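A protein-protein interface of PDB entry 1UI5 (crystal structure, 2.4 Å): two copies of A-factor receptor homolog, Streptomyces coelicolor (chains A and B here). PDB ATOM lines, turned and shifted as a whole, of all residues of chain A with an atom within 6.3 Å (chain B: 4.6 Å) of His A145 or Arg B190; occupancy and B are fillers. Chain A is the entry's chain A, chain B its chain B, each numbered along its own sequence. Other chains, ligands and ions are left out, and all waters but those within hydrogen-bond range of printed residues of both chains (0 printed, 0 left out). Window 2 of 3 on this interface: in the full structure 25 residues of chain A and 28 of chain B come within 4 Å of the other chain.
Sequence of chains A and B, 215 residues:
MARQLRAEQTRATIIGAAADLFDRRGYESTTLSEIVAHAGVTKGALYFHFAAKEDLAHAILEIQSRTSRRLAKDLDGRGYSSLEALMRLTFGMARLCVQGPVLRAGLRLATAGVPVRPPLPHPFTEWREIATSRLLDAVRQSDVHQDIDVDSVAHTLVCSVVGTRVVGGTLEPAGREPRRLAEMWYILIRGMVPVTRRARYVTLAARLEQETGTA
A ring nitrogen (NE2) of His A145 is in hydrogen-bond range of the guanidinium group (NH2) of Arg B190, at 3.0 Å.
The backbone carbonyl oxygen (O) of Gly B191 lies within hydrogen-bond range of the guanidinium group (NE) of Arg A190 (3.0 Å).
N of His A145 sits at hydrogen-bond distance from O of Met A192 (2.9 Å).
The backbone carbonyl oxygen (O) of Arg A190 lies within hydrogen-bond range of the guanidinium group (NH2) of Arg A198, at 3.4 Å.
O of Arg B190 sits at hydrogen-bond distance from NE of Arg B198.
Among the printed residues, merely in contact across the chains: Gly A191 with Ile B187 (3.3 Å) and Gly A191 with Arg B190 (3.4 Å).
His A145 touches just one residue of chain B: Arg B190.
Arg B190 touches just these residues of chain A: His A145 (3.0 Å) and Gly A191 (3.4 Å).
Printed residues of chain A within 4 Å of Gly B191: Arg A190.
Of the printed residues of chain A, Ile B187 touches Gly A191 (3.3 Å).
Of the printed residues of chain B, Arg A190 touches Gly B191 (3.0 Å).
Printed residues of chain B within 4 Å of Gly A191: Ile B187 and Arg B190.
The nearest printed residue of chain B that does not touch His A145 is Ile B187 (6.9 Å).
The nearest residue of chain A that does not touch Arg B190 is Arg A190 (4.5 Å).
The nearest printed residue of chain B that does not touch Arg A190 is Arg B190 (4.5 Å).
Hydrophobic or aromatic side chains of chain A within 4 Å of the printed part of chain B: His A145.
Among the printed residues, no Asp or Glu carboxylate lies within 4 Å of a Lys or Arg side-chain nitrogen of the other chain.
Arg A190 touches Gly B191, and with the chains exchanged Gly A191 touches Arg B190.
5 positions are printed for both chains.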
ATOM      1  N   VAL A 139       5.876  -1.975 -18.883  1.00  0.00           N
ATOM      2  CA  VAL A 139       7.147  -2.066 -19.612  1.00  0.00           C
ATOM      3  C   VAL A 139       7.985  -3.206 -19.053  1.00  0.00           C
ATOM      4  O   VAL A 139       8.503  -4.004 -19.810  1.00  0.00           O
ATOM      5  CB  VAL A 139       7.975  -0.745 -19.556  1.00  0.00           C
ATOM      6  CG1 VAL A 139       9.444  -0.979 -20.071  1.00  0.00           C
ATOM      7  CG2 VAL A 139       7.294   0.349 -20.330  1.00  0.00           C
ATOM      8  N   SER A 142       6.957  -6.559 -20.090  1.00  0.00           N
ATOM      9  CA  SER A 142       7.126  -6.732 -21.528  1.00  0.00           C
ATOM     10  C   SER A 142       5.836  -6.523 -22.343  1.00  0.00           C
ATOM     11  O   SER A 142       5.738  -6.962 -23.459  1.00  0.00           O
ATOM     12  CB  SER A 142       7.806  -8.089 -21.861  1.00  0.00           C
ATOM     13  OG  SER A 142       9.142  -8.148 -21.341  1.00  0.00           O
ATOM     14  N   ASP A 143       4.848  -5.859 -21.780  1.00  0.00           N
ATOM     15  CA  ASP A 143       3.638  -5.531 -22.524  1.00  0.00           C
ATOM     16  C   ASP A 143       3.702  -4.200 -23.276  1.00  0.00           C
ATOM     17  O   ASP A 143       2.882  -3.992 -24.131  1.00  0.00           O
ATOM     18  CB  ASP A 143       2.445  -5.498 -21.609  1.00  0.00           C
ATOM     19  CG  ASP A 143       2.009  -6.862 -21.196  1.00  0.00           C
ATOM     20  OD1 ASP A 143       2.041  -7.786 -22.028  1.00  0.00           O
ATOM     21  OD2 ASP A 143       1.561  -7.111 -20.067  1.00  0.00           O
ATOM     22  N   VAL A 144       4.655  -3.326 -22.942  1.00  0.00           N
ATOM     23  CA  VAL A 144       4.889  -2.033 -23.601  1.00  0.00           C
ATOM     24  C   VAL A 144       6.412  -1.902 -23.925  1.00  0.00           C
ATOM     25  O   VAL A 144       7.247  -2.272 -23.100  1.00  0.00           O
ATOM     26  CB  VAL A 144       4.407  -0.859 -22.690  1.00  0.00           C
ATOM     27  CG1 VAL A 144       4.943   0.488 -23.173  1.00  0.00           C
ATOM     28  CG2 VAL A 144       2.883  -0.825 -22.596  1.00  0.00           C
ATOM     29  N   HIS A 145       6.768  -1.406 -25.122  1.00  0.00           N
ATOM     30  CA  HIS A 145       8.158  -1.393 -25.568  1.00  0.00           C
ATOM     31  C   HIS A 145       9.035  -0.654 -24.577  1.00  0.00           C
ATOM     32  O   HIS A 145       8.627   0.367 -24.026  1.00  0.00           O
ATOM     33  CB  HIS A 145       8.351  -0.699 -26.922  1.00  0.00           C
ATOM     34  CG  HIS A 145       7.489  -1.216 -28.028  1.00  0.00           C
ATOM     35  ND1 HIS A 145       7.412  -2.552 -28.358  1.00  0.00           N
ATOM     36  CD2 HIS A 145       6.694  -0.559 -28.912  1.00  0.00           C
ATOM     37  CE1 HIS A 145       6.582  -2.697 -29.379  1.00  0.00           C
ATOM     38  NE2 HIS A 145       6.129  -1.502 -29.733  1.00  0.00           N
ATOM     39  N   GLN A 146      10.232  -1.167 -24.380  1.00  0.00           N
ATOM     40  CA  GLN A 146      11.204  -0.588 -23.484  1.00  0.00           C
ATOM     41  C   GLN A 146      11.555   0.874 -23.769  1.00  0.00           C
ATOM     42  O   GLN A 146      11.869   1.604 -22.839  1.00  0.00           O
ATOM     43  CB  GLN A 146      12.504  -1.409 -23.525  1.00  0.00           C
ATOM     44  CG  GLN A 146      12.418  -2.719 -22.769  1.00  0.00           C
ATOM     45  CD  GLN A 146      13.597  -2.950 -21.848  1.00  0.00           C
ATOM     46  OE1 GLN A 146      14.680  -3.347 -22.280  1.00  0.00           O
ATOM     47  NE2 GLN A 146      13.378  -2.714 -20.567  1.00  0.00           N
ATOM     48  N   ASP A 147      11.512   1.291 -25.037  1.00  0.00           N
ATOM     49  CA  ASP A 147      11.964   2.635 -25.417  1.00  0.00           C
ATOM     50  C   ASP A 147      10.841   3.690 -25.380  1.00  0.00           C
ATOM     51  O   ASP A 147      11.052   4.843 -25.691  1.00  0.00           O
ATOM     52  CB  ASP A 147      12.667   2.605 -26.789  1.00  0.00           C
ATOM     53  CG  ASP A 147      11.697   2.385 -27.934  1.00  0.00           C
ATOM     54  OD1 ASP A 147      10.649   1.710 -27.731  1.00  0.00           O
ATOM     55  OD2 ASP A 147      11.900   2.843 -29.088  1.00  0.00           O
ATOM     56  N   ILE A 148       9.653   3.275 -24.963  1.00  0.00           N
ATOM     57  CA  ILE A 148       8.536   4.157 -24.838  1.00  0.00           C
ATOM     58  C   ILE A 148       8.727   5.084 -23.652  1.00  0.00           C
ATOM     59  O   ILE A 148       9.031   4.654 -22.548  1.00  0.00           O
ATOM     60  CB  ILE A 148       7.226   3.341 -24.682  1.00  0.00           C
ATOM     61  CG1 ILE A 148       6.881   2.602 -25.978  1.00  0.00           C
ATOM     62  CG2 ILE A 148       6.072   4.215 -24.294  1.00  0.00           C
ATOM     63  CD1 ILE A 148       6.511   3.475 -27.204  1.00  0.00           C
ATOM     64  N   ASP A 149       8.573   6.367 -23.916  1.00  0.00           N
ATOM     65  CA  ASP A 149       8.535   7.391 -22.892  1.00  0.00           C
ATOM     66  C   ASP A 149       7.173   7.318 -22.162  1.00  0.00           C
ATOM     67  O   ASP A 149       6.190   7.906 -22.579  1.00  0.00           O
ATOM     68  CB  ASP A 149       8.757   8.728 -23.605  1.00  0.00           C
ATOM     69  CG  ASP A 149       8.888   9.868 -22.673  1.00  0.00           C
ATOM     70  OD1 ASP A 149       8.708   9.639 -21.450  1.00  0.00           O
ATOM     71  OD2 ASP A 149       9.144  11.035 -23.076  1.00  0.00           O
ATOM     72  N   VAL A 150       7.118   6.600 -21.055  1.00  0.00           N
ATOM     73  CA  VAL A 150       5.853   6.409 -20.356  1.00  0.00           C
ATOM     74  C   VAL A 150       5.257   7.719 -19.838  1.00  0.00           C
ATOM     75  O   VAL A 150       4.052   7.939 -19.948  1.00  0.00           O
ATOM     76  CB  VAL A 150       5.974   5.402 -19.167  1.00  0.00           C
ATOM     77  CG1 VAL A 150       6.619   4.115 -19.608  1.00  0.00           C
ATOM     78  CG2 VAL A 150       6.757   5.988 -18.033  1.00  0.00           C
ATOM     79  N   ILE A 189      -2.365   0.682 -28.196  1.00  0.00           N
ATOM     80  CA  ILE A 189      -1.956  -0.731 -28.262  1.00  0.00           C
ATOM     81  C   ILE A 189      -1.118  -1.016 -29.528  1.00  0.00           C
ATOM     82  O   ILE A 189      -0.054  -1.632 -29.459  1.00  0.00           O
ATOM     83  CB  ILE A 189      -3.212  -1.665 -28.219  1.00  0.00           C
ATOM     84  CG1 ILE A 189      -3.868  -1.606 -26.829  1.00  0.00           C
ATOM     85  CG2 ILE A 189      -2.817  -3.086 -28.570  1.00  0.00           C
ATOM     86  CD1 ILE A 189      -5.235  -2.200 -26.748  1.00  0.00           C
ATOM     87  N   ARG A 190      -1.601  -0.548 -30.669  1.00  0.00           N
ATOM     88  CA  ARG A 190      -0.904  -0.799 -31.935  1.00  0.00           C
ATOM     89  C   ARG A 190       0.493  -0.189 -31.944  1.00  0.00           C
ATOM     90  O   ARG A 190       1.431  -0.760 -32.481  1.00  0.00           O
ATOM     91  CB  ARG A 190      -1.740  -0.317 -33.135  1.00  0.00           C
ATOM     92  CG  ARG A 190      -3.049  -1.149 -33.346  1.00  0.00           C
ATOM     93  CD  ARG A 190      -3.950  -0.742 -34.550  1.00  0.00           C
ATOM     94  NE  ARG A 190      -3.232  -0.714 -35.830  1.00  0.00           N
ATOM     95  CZ  ARG A 190      -2.777  -1.792 -36.479  1.00  0.00           C
ATOM     96  NH1 ARG A 190      -2.981  -3.015 -35.989  1.00  0.00           N
ATOM     97  NH2 ARG A 190      -2.113  -1.656 -37.629  1.00  0.00           N
ATOM     98  N   GLY A 191       0.625   0.937 -31.266  1.00  0.00           N
ATOM     99  CA  GLY A 191       1.840   1.709 -31.260  1.00  0.00           C
ATOM    100  C   GLY A 191       2.775   1.434 -30.121  1.00  0.00           C
ATOM    101  O   GLY A 191       3.953   1.649 -30.286  1.00  0.00           O
ATOM    102  N   MET A 192       2.401   0.779 -29.068  1.00  0.00           N
ATOM    103  CA  MET A 192       3.334   0.734 -27.952  1.00  0.00           C
ATOM    104  C   MET A 192       3.399  -0.669 -27.409  1.00  0.00           C
ATOM    105  O   MET A 192       4.301  -0.998 -26.645  1.00  0.00           O
ATOM    106  CB  MET A 192       2.928   1.722 -26.858  1.00  0.00           C
ATOM    107  CG  MET A 192       1.862   1.266 -25.926  1.00  0.00           C
ATOM    108  SD  MET A 192       1.339   2.700 -24.676  1.00  0.00           S
ATOM    109  CE  MET A 192      -0.032   1.750 -23.763  1.00  0.00           C
ATOM    110  N   VAL A 193       2.672  -1.643 -27.930  1.00  0.00           N
ATOM    111  CA  VAL A 193       2.578  -3.021 -27.372  1.00  0.00           C
ATOM    112  C   VAL A 193       3.244  -3.910 -28.372  1.00  0.00           C
ATOM    113  O   VAL A 193       2.932  -3.813 -29.538  1.00  0.00           O
ATOM    114  CB  VAL A 193       1.106  -3.469 -27.189  1.00  0.00           C
ATOM    115  CG1 VAL A 193       1.034  -4.933 -26.829  1.00  0.00           C
ATOM    116  CG2 VAL A 193       0.391  -2.617 -26.130  1.00  0.00           C
ATOM    117  N   PRO A 194       4.175  -4.755 -27.956  1.00  0.00           N
ATOM    118  CA  PRO A 194       4.840  -5.672 -28.910  1.00  0.00           C
ATOM    119  C   PRO A 194       3.789  -6.503 -29.665  1.00  0.00           C
ATOM    120  O   PRO A 194       2.745  -6.872 -29.098  1.00  0.00           O
ATOM    121  CB  PRO A 194       5.734  -6.542 -28.036  1.00  0.00           C
ATOM    122  CG  PRO A 194       5.907  -5.744 -26.746  1.00  0.00           C
ATOM    123  CD  PRO A 194       4.657  -4.918 -26.580  1.00  0.00           C
ATOM    124  N   VAL A 195       4.087  -6.754 -30.945  1.00  0.00           N
ATOM    125  CA  VAL A 195       3.176  -7.348 -31.875  1.00  0.00           C
ATOM    126  C   VAL A 195       2.592  -8.638 -31.388  1.00  0.00           C
ATOM    127  O   VAL A 195       1.448  -8.882 -31.685  1.00  0.00           O
ATOM    128  CB  VAL A 195       3.830  -7.564 -33.254  1.00  0.00           C
ATOM    129  CG1 VAL A 195       4.899  -8.654 -33.186  1.00  0.00           C
ATOM    130  CG2 VAL A 195       2.755  -7.920 -34.311  1.00  0.00           C
ATOM    131  N   ARG A 198      -0.092  -8.140 -28.728  1.00  0.00           N
ATOM    132  CA  ARG A 198      -1.104  -7.200 -29.227  1.00  0.00           C
ATOM    133  C   ARG A 198      -2.585  -7.614 -29.256  1.00  0.00           C
ATOM    134  O   ARG A 198      -3.456  -6.905 -28.753  1.00  0.00           O
ATOM    135  CB  ARG A 198      -0.698  -6.744 -30.634  1.00  0.00           C
ATOM    136  CG  ARG A 198      -1.410  -5.495 -31.122  1.00  0.00           C
ATOM    137  CD  ARG A 198      -0.794  -4.872 -32.418  1.00  0.00           C
ATOM    138  NE  ARG A 198       0.632  -4.588 -32.260  1.00  0.00           N
ATOM    139  CZ  ARG A 198       1.410  -4.063 -33.205  1.00  0.00           C
ATOM    140  NH1 ARG A 198       0.908  -3.714 -34.386  1.00  0.00           N
ATOM    141  NH2 ARG A 198       2.695  -3.851 -32.953  1.00  0.00           N
ATOM    142  N   TYR B 186       5.440   8.878 -32.833  1.00  0.00           N
ATOM    143  CA  TYR B 186       6.044   7.540 -32.906  1.00  0.00           C
ATOM    144  C   TYR B 186       4.967   6.417 -32.733  1.00  0.00           C
ATOM    145  O   TYR B 186       4.972   5.453 -33.466  1.00  0.00           O
ATOM    146  CB  TYR B 186       7.154   7.294 -31.847  1.00  0.00           C
ATOM    147  CG  TYR B 186       8.289   8.296 -31.728  1.00  0.00           C
ATOM    148  CD1 TYR B 186       8.654   9.131 -32.791  1.00  0.00           C
ATOM    149  CD2 TYR B 186       9.060   8.374 -30.545  1.00  0.00           C
ATOM    150  CE1 TYR B 186       9.705  10.024 -32.688  1.00  0.00           C
ATOM    151  CE2 TYR B 186      10.106   9.250 -30.433  1.00  0.00           C
ATOM    152  CZ  TYR B 186      10.435  10.104 -31.518  1.00  0.00           C
ATOM    153  OH  TYR B 186      11.500  11.043 -31.438  1.00  0.00           O
ATOM    154  N   ILE B 187       4.064   6.580 -31.771  1.00  0.00           N
ATOM    155  CA  ILE B 187       3.064   5.583 -31.464  1.00  0.00           C
ATOM    156  C   ILE B 187       2.083   5.514 -32.589  1.00  0.00           C
ATOM    157  O   ILE B 187       1.714   4.427 -33.047  1.00  0.00           O
ATOM    158  CB  ILE B 187       2.367   5.874 -30.130  1.00  0.00           C
ATOM    159  CG1 ILE B 187       3.268   5.455 -28.973  1.00  0.00           C
ATOM    160  CG2 ILE B 187       1.038   5.114 -30.028  1.00  0.00           C
ATOM    161  CD1 ILE B 187       2.942   6.008 -27.620  1.00  0.00           C
ATOM    162  N   LEU B 188       1.667   6.675 -33.050  1.00  0.00           N
ATOM    163  CA  LEU B 188       0.703   6.739 -34.149  1.00  0.00           C
ATOM    164  C   LEU B 188       1.268   6.128 -35.391  1.00  0.00           C
ATOM    165  O   LEU B 188       0.556   5.404 -36.076  1.00  0.00           O
ATOM    166  CB  LEU B 188       0.326   8.179 -34.460  1.00  0.00           C
ATOM    167  CG  LEU B 188      -0.600   8.802 -33.437  1.00  0.00           C
ATOM    168  CD1 LEU B 188      -0.713  10.364 -33.583  1.00  0.00           C
ATOM    169  CD2 LEU B 188      -1.979   8.144 -33.483  1.00  0.00           C
ATOM    170  N   ILE B 189       2.556   6.425 -35.677  1.00  0.00           N
ATOM    171  CA  ILE B 189       3.224   5.986 -36.926  1.00  0.00           C
ATOM    172  C   ILE B 189       3.355   4.479 -36.944  1.00  0.00           C
ATOM    173  O   ILE B 189       3.099   3.819 -37.958  1.00  0.00           O
ATOM    174  CB  ILE B 189       4.652   6.656 -37.085  1.00  0.00           C
ATOM    175  CG1 ILE B 189       4.527   8.152 -37.391  1.00  0.00           C
ATOM    176  CG2 ILE B 189       5.439   6.013 -38.199  1.00  0.00           C
ATOM    177  CD1 ILE B 189       5.753   8.979 -37.059  1.00  0.00           C
ATOM    178  N   ARG B 190       3.813   3.935 -35.843  1.00  0.00           N
ATOM    179  CA  ARG B 190       3.908   2.497 -35.673  1.00  0.00           C
ATOM    180  C   ARG B 190       2.548   1.820 -35.937  1.00  0.00           C
ATOM    181  O   ARG B 190       2.490   0.758 -36.543  1.00  0.00           O
ATOM    182  CB  ARG B 190       4.392   2.155 -34.237  1.00  0.00           C
ATOM    183  CG  ARG B 190       5.884   2.262 -34.040  1.00  0.00           C
ATOM    184  CD  ARG B 190       6.368   1.828 -32.643  1.00  0.00           C
ATOM    185  NE  ARG B 190       6.386   0.365 -32.495  1.00  0.00           N
ATOM    186  CZ  ARG B 190       7.446  -0.426 -32.662  1.00  0.00           C
ATOM    187  NH1 ARG B 190       8.632   0.078 -32.995  1.00  0.00           N
ATOM    188  NH2 ARG B 190       7.325  -1.742 -32.489  1.00  0.00           N
ATOM    189  N   GLY B 191       1.451   2.467 -35.540  1.00  0.00           N
ATOM    190  CA  GLY B 191       0.138   1.837 -35.615  1.00  0.00           C
ATOM    191  C   GLY B 191      -0.660   2.090 -36.875  1.00  0.00           C
ATOM    192  O   GLY B 191      -1.582   1.354 -37.165  1.00  0.00           O
ATOM    193  N   MET B 192      -0.368   3.193 -37.687  1.00  0.00           N
ATOM    194  CA  MET B 192      -1.257   3.561 -38.771  1.00  0.00           C
ATOM    195  C   MET B 192      -0.499   3.810 -40.062  1.00  0.00           C
ATOM    196  O   MET B 192      -1.087   4.030 -41.109  1.00  0.00           O
ATOM    197  CB  MET B 192      -2.039   4.813 -38.377  1.00  0.00           C
ATOM    198  CG  MET B 192      -1.295   6.135 -38.517  1.00  0.00           C
ATOM    199  SD  MET B 192      -2.412   7.646 -37.887  1.00  0.00           S
ATOM    200  CE  MET B 192      -2.916   6.850 -36.200  1.00  0.00           C
ATOM    201  N   ARG B 198       7.098   3.645 -42.908  1.00  0.00           N
ATOM    202  CA  ARG B 198       7.283   4.073 -41.509  1.00  0.00           C
ATOM    203  C   ARG B 198       8.597   4.808 -41.275  1.00  0.00           C
ATOM    204  O   ARG B 198       8.635   5.868 -40.685  1.00  0.00           O
ATOM    205  CB  ARG B 198       7.288   2.891 -40.560  1.00  0.00           C
ATOM    206  CG  ARG B 198       5.954   2.289 -40.359  1.00  0.00           C
ATOM    207  CD  ARG B 198       5.750   1.470 -39.054  1.00  0.00           C
ATOM    208  NE  ARG B 198       4.507   0.742 -39.277  1.00  0.00           N
ATOM    209  CZ  ARG B 198       4.373  -0.583 -39.217  1.00  0.00           C
ATOM    210  NH1 ARG B 198       5.400  -1.371 -38.885  1.00  0.00           N
ATOM    211  NH2 ARG B 198       3.201  -1.128 -39.485  1.00  0.00           N
